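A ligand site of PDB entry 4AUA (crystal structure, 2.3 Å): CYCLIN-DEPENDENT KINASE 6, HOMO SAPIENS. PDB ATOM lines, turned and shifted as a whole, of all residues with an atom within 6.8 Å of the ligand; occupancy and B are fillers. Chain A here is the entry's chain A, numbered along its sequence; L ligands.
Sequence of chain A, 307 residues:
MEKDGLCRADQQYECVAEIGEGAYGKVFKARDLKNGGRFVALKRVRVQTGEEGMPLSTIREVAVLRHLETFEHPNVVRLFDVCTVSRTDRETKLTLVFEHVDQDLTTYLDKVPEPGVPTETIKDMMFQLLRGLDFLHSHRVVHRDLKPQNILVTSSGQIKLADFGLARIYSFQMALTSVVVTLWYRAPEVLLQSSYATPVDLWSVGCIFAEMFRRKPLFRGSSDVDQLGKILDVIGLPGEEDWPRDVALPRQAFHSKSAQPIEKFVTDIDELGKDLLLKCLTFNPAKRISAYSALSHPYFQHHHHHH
N of Val 101 is in hydrogen-bond range of O1 of the ligand, at 3.0 Å.
The backbone carbonyl oxygen (O) of Val 101 sits close to a nitrogen (N3) of the ligand (2.8 Å).
The backbone carbonyl oxygen (O) of Glu 99 lies within hydrogen-bond range of a nitrogen (N2) of the ligand.
The side-chain carboxylate (OD1) of Asp 104 is in hydrogen-bond range of the side-chain hydroxyl (OG1) of Thr 107 (2.8 Å).
N of Thr 106 lies close to OD1 of Asp 104, 3.2 Å away.
O of Val 27 is in hydrogen-bond range of N of Ile 19, 3.0 Å away.
O of Arg 78 is in hydrogen-bond range of N of Glu 99, at 2.9 Å.
The backbone carbonyl oxygen (O) of Ala 41 is in hydrogen-bond range of the backbone NH (N) of Phe 98 (2.9 Å).
The backbone carbonyl oxygen (O) of Asn 150 is in hydrogen-bond range of the backbone NH (N) of Ala 162, at 3.0 Å.
Residues that only touch the ligand: Asp 104, Ile 19, Asp 102, Ala 41, His 100, Leu 152, Ala 162 and Gln 103.
Of the 24 residues printed, 10 come within 4 Å of the ligand.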
ATOM      1  N   ILE A  19     -12.954  15.885   1.648  1.00  0.00           N
ATOM      2  CA  ILE A  19     -13.601  16.871   0.742  1.00  0.00           C
ATOM      3  C   ILE A  19     -13.393  18.417   0.913  1.00  0.00           C
ATOM      4  O   ILE A  19     -13.842  19.160   0.046  1.00  0.00           O
ATOM      5  CB  ILE A  19     -15.129  16.605   0.662  1.00  0.00           C
ATOM      6  CG1 ILE A  19     -15.816  16.892   2.008  1.00  0.00           C
ATOM      7  CG2 ILE A  19     -15.404  15.173   0.240  1.00  0.00           C
ATOM      8  CD1 ILE A  19     -17.314  16.742   1.952  1.00  0.00           C
ATOM      9  N   GLY A  20     -12.738  18.917   1.966  1.00  0.00           N
ATOM     10  CA  GLY A  20     -12.115  18.128   3.005  1.00  0.00           C
ATOM     11  C   GLY A  20     -11.563  18.913   4.184  1.00  0.00           C
ATOM     12  O   GLY A  20     -12.001  18.692   5.317  1.00  0.00           O
ATOM     13  N   VAL A  27     -13.199  17.088   6.861  1.00  0.00           N
ATOM     14  CA  VAL A  27     -14.550  16.708   6.456  1.00  0.00           C
ATOM     15  C   VAL A  27     -14.438  15.470   5.573  1.00  0.00           C
ATOM     16  O   VAL A  27     -13.747  15.502   4.547  1.00  0.00           O
ATOM     17  CB  VAL A  27     -15.232  17.821   5.644  1.00  0.00           C
ATOM     18  CG1 VAL A  27     -16.627  17.397   5.227  1.00  0.00           C
ATOM     19  CG2 VAL A  27     -15.268  19.123   6.446  1.00  0.00           C
ATOM     20  N   VAL A  40     -22.787  10.743   2.938  1.00  0.00           N
ATOM     21  CA  VAL A  40     -22.846  11.809   3.953  1.00  0.00           C
ATOM     22  C   VAL A  40     -21.479  12.525   4.091  1.00  0.00           C
ATOM     23  O   VAL A  40     -20.494  12.134   3.475  1.00  0.00           O
ATOM     24  CB  VAL A  40     -23.262  11.234   5.320  1.00  0.00           C
ATOM     25  CG1 VAL A  40     -24.710  10.726   5.251  1.00  0.00           C
ATOM     26  CG2 VAL A  40     -22.324  10.107   5.729  1.00  0.00           C
ATOM     27  N   ALA A  41     -21.450  13.585   4.880  1.00  0.00           N
ATOM     28  CA  ALA A  41     -20.220  14.264   5.254  1.00  0.00           C
ATOM     29  C   ALA A  41     -20.015  14.126   6.763  1.00  0.00           C
ATOM     30  O   ALA A  41     -20.784  14.704   7.537  1.00  0.00           O
ATOM     31  CB  ALA A  41     -20.283  15.757   4.860  1.00  0.00           C
ATOM     32  N   LEU A  42     -19.015  13.350   7.180  1.00  0.00           N
ATOM     33  CA  LEU A  42     -18.675  13.157   8.598  1.00  0.00           C
ATOM     34  C   LEU A  42     -17.635  14.184   9.105  1.00  0.00           C
ATOM     35  O   LEU A  42     -16.646  14.463   8.424  1.00  0.00           O
ATOM     36  CB  LEU A  42     -18.102  11.753   8.819  1.00  0.00           C
ATOM     37  CG  LEU A  42     -18.985  10.533   8.530  1.00  0.00           C
ATOM     38  CD1 LEU A  42     -18.111   9.279   8.379  1.00  0.00           C
ATOM     39  CD2 LEU A  42     -20.010  10.328   9.626  1.00  0.00           C
ATOM     40  N   LYS A  43     -17.853  14.700  10.313  1.00  0.00           N
ATOM     41  CA  LYS A  43     -17.001  15.752  10.900  1.00  0.00           C
ATOM     42  C   LYS A  43     -16.592  15.377  12.325  1.00  0.00           C
ATOM     43  O   LYS A  43     -17.436  15.124  13.164  1.00  0.00           O
ATOM     44  CB  LYS A  43     -17.767  17.078  10.922  1.00  0.00           C
ATOM     45  CG  LYS A  43     -16.929  18.307  11.283  1.00  0.00           C
ATOM     46  CD  LYS A  43     -17.760  19.509  11.738  1.00  0.00           C
ATOM     47  CE  LYS A  43     -18.365  20.311  10.573  1.00  0.00           C
ATOM     48  NZ  LYS A  43     -18.914  21.646  10.989  1.00  0.00           N
ATOM     49  N   VAL A  77     -27.313  23.027   5.238  1.00  0.00           N
ATOM     50  CA  VAL A  77     -27.027  21.613   5.152  1.00  0.00           C
ATOM     51  C   VAL A  77     -27.854  20.927   6.251  1.00  0.00           C
ATOM     52  O   VAL A  77     -28.060  21.494   7.332  1.00  0.00           O
ATOM     53  CB  VAL A  77     -25.480  21.374   5.241  1.00  0.00           C
ATOM     54  CG1 VAL A  77     -24.923  21.608   6.660  1.00  0.00           C
ATOM     55  CG2 VAL A  77     -25.095  20.029   4.763  1.00  0.00           C
ATOM     56  N   ARG A  78     -28.370  19.735   5.943  1.00  0.00           N
ATOM     57  CA  ARG A  78     -29.096  18.929   6.929  1.00  0.00           C
ATOM     58  C   ARG A  78     -28.096  18.306   7.883  1.00  0.00           C
ATOM     59  O   ARG A  78     -27.060  17.797   7.446  1.00  0.00           O
ATOM     60  CB  ARG A  78     -29.889  17.798   6.258  1.00  0.00           C
ATOM     61  CG  ARG A  78     -31.028  18.200   5.298  1.00  0.00           C
ATOM     62  CD  ARG A  78     -32.278  18.601   6.055  1.00  0.00           C
ATOM     63  NE  ARG A  78     -32.022  19.837   6.794  1.00  0.00           N
ATOM     64  CZ  ARG A  78     -32.148  21.066   6.300  1.00  0.00           C
ATOM     65  NH1 ARG A  78     -32.587  21.248   5.056  1.00  0.00           N
ATOM     66  NH2 ARG A  78     -31.846  22.107   7.052  1.00  0.00           N
ATOM     67  N   PHE A  98     -23.523  15.082   8.467  1.00  0.00           N
ATOM     68  CA  PHE A  98     -24.291  16.022   7.672  1.00  0.00           C
ATOM     69  C   PHE A  98     -24.632  15.467   6.309  1.00  0.00           C
ATOM     70  O   PHE A  98     -24.075  14.468   5.856  1.00  0.00           O
ATOM     71  CB  PHE A  98     -23.505  17.308   7.425  1.00  0.00           C
ATOM     72  CG  PHE A  98     -23.220  18.094   8.653  1.00  0.00           C
ATOM     73  CD1 PHE A  98     -24.130  19.015   9.126  1.00  0.00           C
ATOM     74  CD2 PHE A  98     -22.014  17.939   9.340  1.00  0.00           C
ATOM     75  CE1 PHE A  98     -23.864  19.750  10.264  1.00  0.00           C
ATOM     76  CE2 PHE A  98     -21.738  18.674  10.481  1.00  0.00           C
ATOM     77  CZ  PHE A  98     -22.660  19.568  10.945  1.00  0.00           C
ATOM     78  N   GLU A  99     -25.528  16.189   5.653  1.00  0.00           N
ATOM     79  CA  GLU A  99     -25.815  16.028   4.268  1.00  0.00           C
ATOM     80  C   GLU A  99     -24.581  16.285   3.380  1.00  0.00           C
ATOM     81  O   GLU A  99     -23.927  17.359   3.495  1.00  0.00           O
ATOM     82  CB  GLU A  99     -26.845  17.090   3.912  1.00  0.00           C
ATOM     83  CG  GLU A  99     -27.452  16.963   2.549  1.00  0.00           C
ATOM     84  CD  GLU A  99     -28.318  18.145   2.220  1.00  0.00           C
ATOM     85  OE1 GLU A  99     -28.517  19.025   3.110  1.00  0.00           O
ATOM     86  OE2 GLU A  99     -28.779  18.202   1.056  1.00  0.00           O
ATOM     87  N   HIS A 100     -24.295  15.343   2.483  1.00  0.00           N
ATOM     88  CA  HIS A 100     -23.294  15.543   1.447  1.00  0.00           C
ATOM     89  C   HIS A 100     -23.914  16.124   0.172  1.00  0.00           C
ATOM     90  O   HIS A 100     -24.935  15.627  -0.306  1.00  0.00           O
ATOM     91  CB  HIS A 100     -22.599  14.218   1.127  1.00  0.00           C
ATOM     92  CG  HIS A 100     -21.701  14.309  -0.068  1.00  0.00           C
ATOM     93  ND1 HIS A 100     -20.389  14.737   0.012  1.00  0.00           N
ATOM     94  CD2 HIS A 100     -21.929  14.078  -1.387  1.00  0.00           C
ATOM     95  CE1 HIS A 100     -19.850  14.742  -1.196  1.00  0.00           C
ATOM     96  NE2 HIS A 100     -20.767  14.350  -2.065  1.00  0.00           N
ATOM     97  N   VAL A 101     -23.299  17.179  -0.379  1.00  0.00           N
ATOM     98  CA  VAL A 101     -23.627  17.681  -1.721  1.00  0.00           C
ATOM     99  C   VAL A 101     -22.393  17.632  -2.637  1.00  0.00           C
ATOM    100  O   VAL A 101     -21.289  17.824  -2.189  1.00  0.00           O
ATOM    101  CB  VAL A 101     -24.393  19.056  -1.719  1.00  0.00           C
ATOM    102  CG1 VAL A 101     -24.562  19.632  -0.315  1.00  0.00           C
ATOM    103  CG2 VAL A 101     -23.790  20.057  -2.692  1.00  0.00           C
ATOM    104  N   ASP A 102     -22.595  17.284  -3.900  1.00  0.00           N
ATOM    105  CA  ASP A 102     -21.495  16.991  -4.818  1.00  0.00           C
ATOM    106  C   ASP A 102     -20.537  18.151  -5.021  1.00  0.00           C
ATOM    107  O   ASP A 102     -19.335  17.938  -5.090  1.00  0.00           O
ATOM    108  CB  ASP A 102     -22.016  16.533  -6.194  1.00  0.00           C
ATOM    109  CG  ASP A 102     -22.510  15.096  -6.208  1.00  0.00           C
ATOM    110  OD1 ASP A 102     -21.996  14.288  -5.400  1.00  0.00           O
ATOM    111  OD2 ASP A 102     -23.407  14.773  -7.036  1.00  0.00           O
ATOM    112  N   GLN A 103     -21.046  19.372  -5.162  1.00  0.00           N
ATOM    113  CA  GLN A 103     -20.125  20.497  -5.263  1.00  0.00           C
ATOM    114  C   GLN A 103     -20.354  21.663  -4.312  1.00  0.00           C
ATOM    115  O   GLN A 103     -21.391  21.779  -3.655  1.00  0.00           O
ATOM    116  CB  GLN A 103     -19.959  20.987  -6.714  1.00  0.00           C
ATOM    117  CG  GLN A 103     -21.173  21.104  -7.582  1.00  0.00           C
ATOM    118  CD  GLN A 103     -20.827  20.802  -9.034  1.00  0.00           C
ATOM    119  OE1 GLN A 103     -20.989  21.666  -9.918  1.00  0.00           O
ATOM    120  NE2 GLN A 103     -20.327  19.592  -9.286  1.00  0.00           N
ATOM    121  N   ASP A 104     -19.302  22.482  -4.232  1.00  0.00           N
ATOM    122  CA  ASP A 104     -19.335  23.781  -3.547  1.00  0.00           C
ATOM    123  C   ASP A 104     -19.269  24.903  -4.584  1.00  0.00           C
ATOM    124  O   ASP A 104     -19.145  24.646  -5.781  1.00  0.00           O
ATOM    125  CB  ASP A 104     -18.160  23.866  -2.565  1.00  0.00           C
ATOM    126  CG  ASP A 104     -16.801  23.811  -3.245  1.00  0.00           C
ATOM    127  OD1 ASP A 104     -16.735  23.926  -4.488  1.00  0.00           O
ATOM    128  OD2 ASP A 104     -15.796  23.651  -2.532  1.00  0.00           O
ATOM    129  N   LEU A 105     -19.352  26.139  -4.140  1.00  0.00           N
ATOM    130  CA  LEU A 105     -19.431  27.263  -5.075  1.00  0.00           C
ATOM    131  C   LEU A 105     -18.126  27.419  -5.864  1.00  0.00           C
ATOM    132  O   LEU A 105     -18.143  27.878  -6.994  1.00  0.00           O
ATOM    133  CB  LEU A 105     -19.750  28.567  -4.346  1.00  0.00           C
ATOM    134  CG  LEU A 105     -20.797  29.530  -4.927  1.00  0.00           C
ATOM    135  CD1 LEU A 105     -20.425  30.959  -4.528  1.00  0.00           C
ATOM    136  CD2 LEU A 105     -20.977  29.428  -6.445  1.00  0.00           C
ATOM    137  N   THR A 106     -17.015  27.040  -5.247  1.00  0.00           N
ATOM    138  CA  THR A 106     -15.685  27.137  -5.850  1.00  0.00           C
ATOM    139  C   THR A 106     -15.655  26.315  -7.123  1.00  0.00           C
ATOM    140  O   THR A 106     -15.357  26.833  -8.204  1.00  0.00           O
ATOM    141  CB  THR A 106     -14.590  26.608  -4.898  1.00  0.00           C
ATOM    142  OG1 THR A 106     -14.438  27.515  -3.801  1.00  0.00           O
ATOM    143  CG2 THR A 106     -13.243  26.470  -5.621  1.00  0.00           C
ATOM    144  N   THR A 107     -15.977  25.026  -6.984  1.00  0.00           N
ATOM    145  CA  THR A 107     -15.990  24.096  -8.119  1.00  0.00           C
ATOM    146  C   THR A 107     -17.044  24.455  -9.172  1.00  0.00           C
ATOM    147  O   THR A 107     -16.853  24.243 -10.367  1.00  0.00           O
ATOM    148  CB  THR A 107     -16.192  22.652  -7.659  1.00  0.00           C
ATOM    149  OG1 THR A 107     -17.382  22.583  -6.876  1.00  0.00           O
ATOM    150  CG2 THR A 107     -15.007  22.197  -6.803  1.00  0.00           C
ATOM    151  N   GLN A 149     -16.211  27.822  -0.480  1.00  0.00           N
ATOM    152  CA  GLN A 149     -15.849  26.451  -0.116  1.00  0.00           C
ATOM    153  C   GLN A 149     -16.830  25.769   0.830  1.00  0.00           C
ATOM    154  O   GLN A 149     -16.822  24.546   0.956  1.00  0.00           O
ATOM    155  CB  GLN A 149     -14.500  26.443   0.614  1.00  0.00           C
ATOM    156  CG  GLN A 149     -13.286  26.521  -0.280  1.00  0.00           C
ATOM    157  CD  GLN A 149     -13.013  27.903  -0.871  1.00  0.00           C
ATOM    158  OE1 GLN A 149     -12.566  28.003  -2.021  1.00  0.00           O
ATOM    159  NE2 GLN A 149     -13.260  28.970  -0.086  1.00  0.00           N
ATOM    160  N   ASN A 150     -17.603  26.561   1.559  1.00  0.00           N
ATOM    161  CA  ASN A 150     -18.649  26.016   2.407  1.00  0.00           C
ATOM    162  C   ASN A 150     -20.025  26.596   2.045  1.00  0.00           C
ATOM    163  O   ASN A 150     -20.932  26.622   2.862  1.00  0.00           O
ATOM    164  CB  ASN A 150     -18.297  26.199   3.893  1.00  0.00           C
ATOM    165  CG  ASN A 150     -18.066  27.648   4.286  1.00  0.00           C
ATOM    166  OD1 ASN A 150     -18.712  28.570   3.782  1.00  0.00           O
ATOM    167  ND2 ASN A 150     -17.160  27.840   5.236  1.00  0.00           N
ATOM    168  N   LEU A 152     -22.664  25.331  -0.563  1.00  0.00           N
ATOM    169  CA  LEU A 152     -22.812  24.109  -1.369  1.00  0.00           C
ATOM    170  C   LEU A 152     -23.890  24.287  -2.415  1.00  0.00           C
ATOM    171  O   LEU A 152     -24.865  25.002  -2.201  1.00  0.00           O
ATOM    172  CB  LEU A 152     -23.026  22.892  -0.470  1.00  0.00           C
ATOM    173  CG  LEU A 152     -21.885  22.680   0.546  1.00  0.00           C
ATOM    174  CD1 LEU A 152     -22.245  21.611   1.546  1.00  0.00           C
ATOM    175  CD2 LEU A 152     -20.531  22.360  -0.118  1.00  0.00           C
ATOM    176  N   ALA A 162     -22.930  25.471   4.812  1.00  0.00           N
ATOM    177  CA  ALA A 162     -22.310  24.498   5.706  1.00  0.00           C
ATOM    178  C   ALA A 162     -21.255  25.164   6.570  1.00  0.00           C
ATOM    179  O   ALA A 162     -20.863  26.309   6.305  1.00  0.00           O
ATOM    180  CB  ALA A 162     -21.655  23.380   4.910  1.00  0.00           C
ATOM    181  N   ASP A 163     -20.813  24.434   7.571  1.00  0.00           N
ATOM    182  CA  ASP A 163     -19.622  24.749   8.369  1.00  0.00           C
ATOM    183  C   ASP A 163     -19.800  25.970   9.255  1.00  0.00           C
ATOM    184  O   ASP A 163     -18.904  26.804   9.353  1.00  0.00           O
ATOM    185  CB  ASP A 163     -18.391  24.879   7.469  1.00  0.00           C
ATOM    186  CG  ASP A 163     -17.216  24.077   7.973  1.00  0.00           C
ATOM    187  OD1 ASP A 163     -17.041  23.976   9.202  1.00  0.00           O
ATOM    188  OD2 ASP A 163     -16.462  23.522   7.134  1.00  0.00           O
HETATM  189  C1  LIG L   1     -16.071  20.711  -1.969  1.00  0.00           C
HETATM  190  C2  LIG L   1     -16.461  20.796  -0.633  1.00  0.00           C
HETATM  191  C3  LIG L   1     -17.605  20.134  -0.226  1.00  0.00           C
HETATM  192  C4  LIG L   1     -18.347  19.412  -1.147  1.00  0.00           C
HETATM  193  C5  LIG L   1     -17.978  19.341  -2.470  1.00  0.00           C
HETATM  194  C6  LIG L   1     -16.834  20.003  -2.877  1.00  0.00           C
HETATM  195  C7  LIG L   1     -19.309  19.283   0.833  1.00  0.00           C
HETATM  196  N1  LIG L   1     -18.199  20.052   1.049  1.00  0.00           N
HETATM  197  C8  LIG L   1     -20.297  18.860   1.824  1.00  0.00           C
HETATM  198  C9  LIG L   1     -20.215  19.363   3.211  1.00  0.00           C
HETATM  199  C10 LIG L   1     -19.369  20.274   3.841  1.00  0.00           C
HETATM  200  C11 LIG L   1     -19.757  20.368   5.172  1.00  0.00           C
HETATM  201  C12 LIG L   1     -20.846  19.495   5.339  1.00  0.00           C
HETATM  202  N2  LIG L   1     -21.105  18.894   4.149  1.00  0.00           N
HETATM  203  N3  LIG L   1     -19.416  18.886  -0.471  1.00  0.00           N
HETATM  204  O1  LIG L   1     -21.169  18.108   1.460  1.00  0.00           O
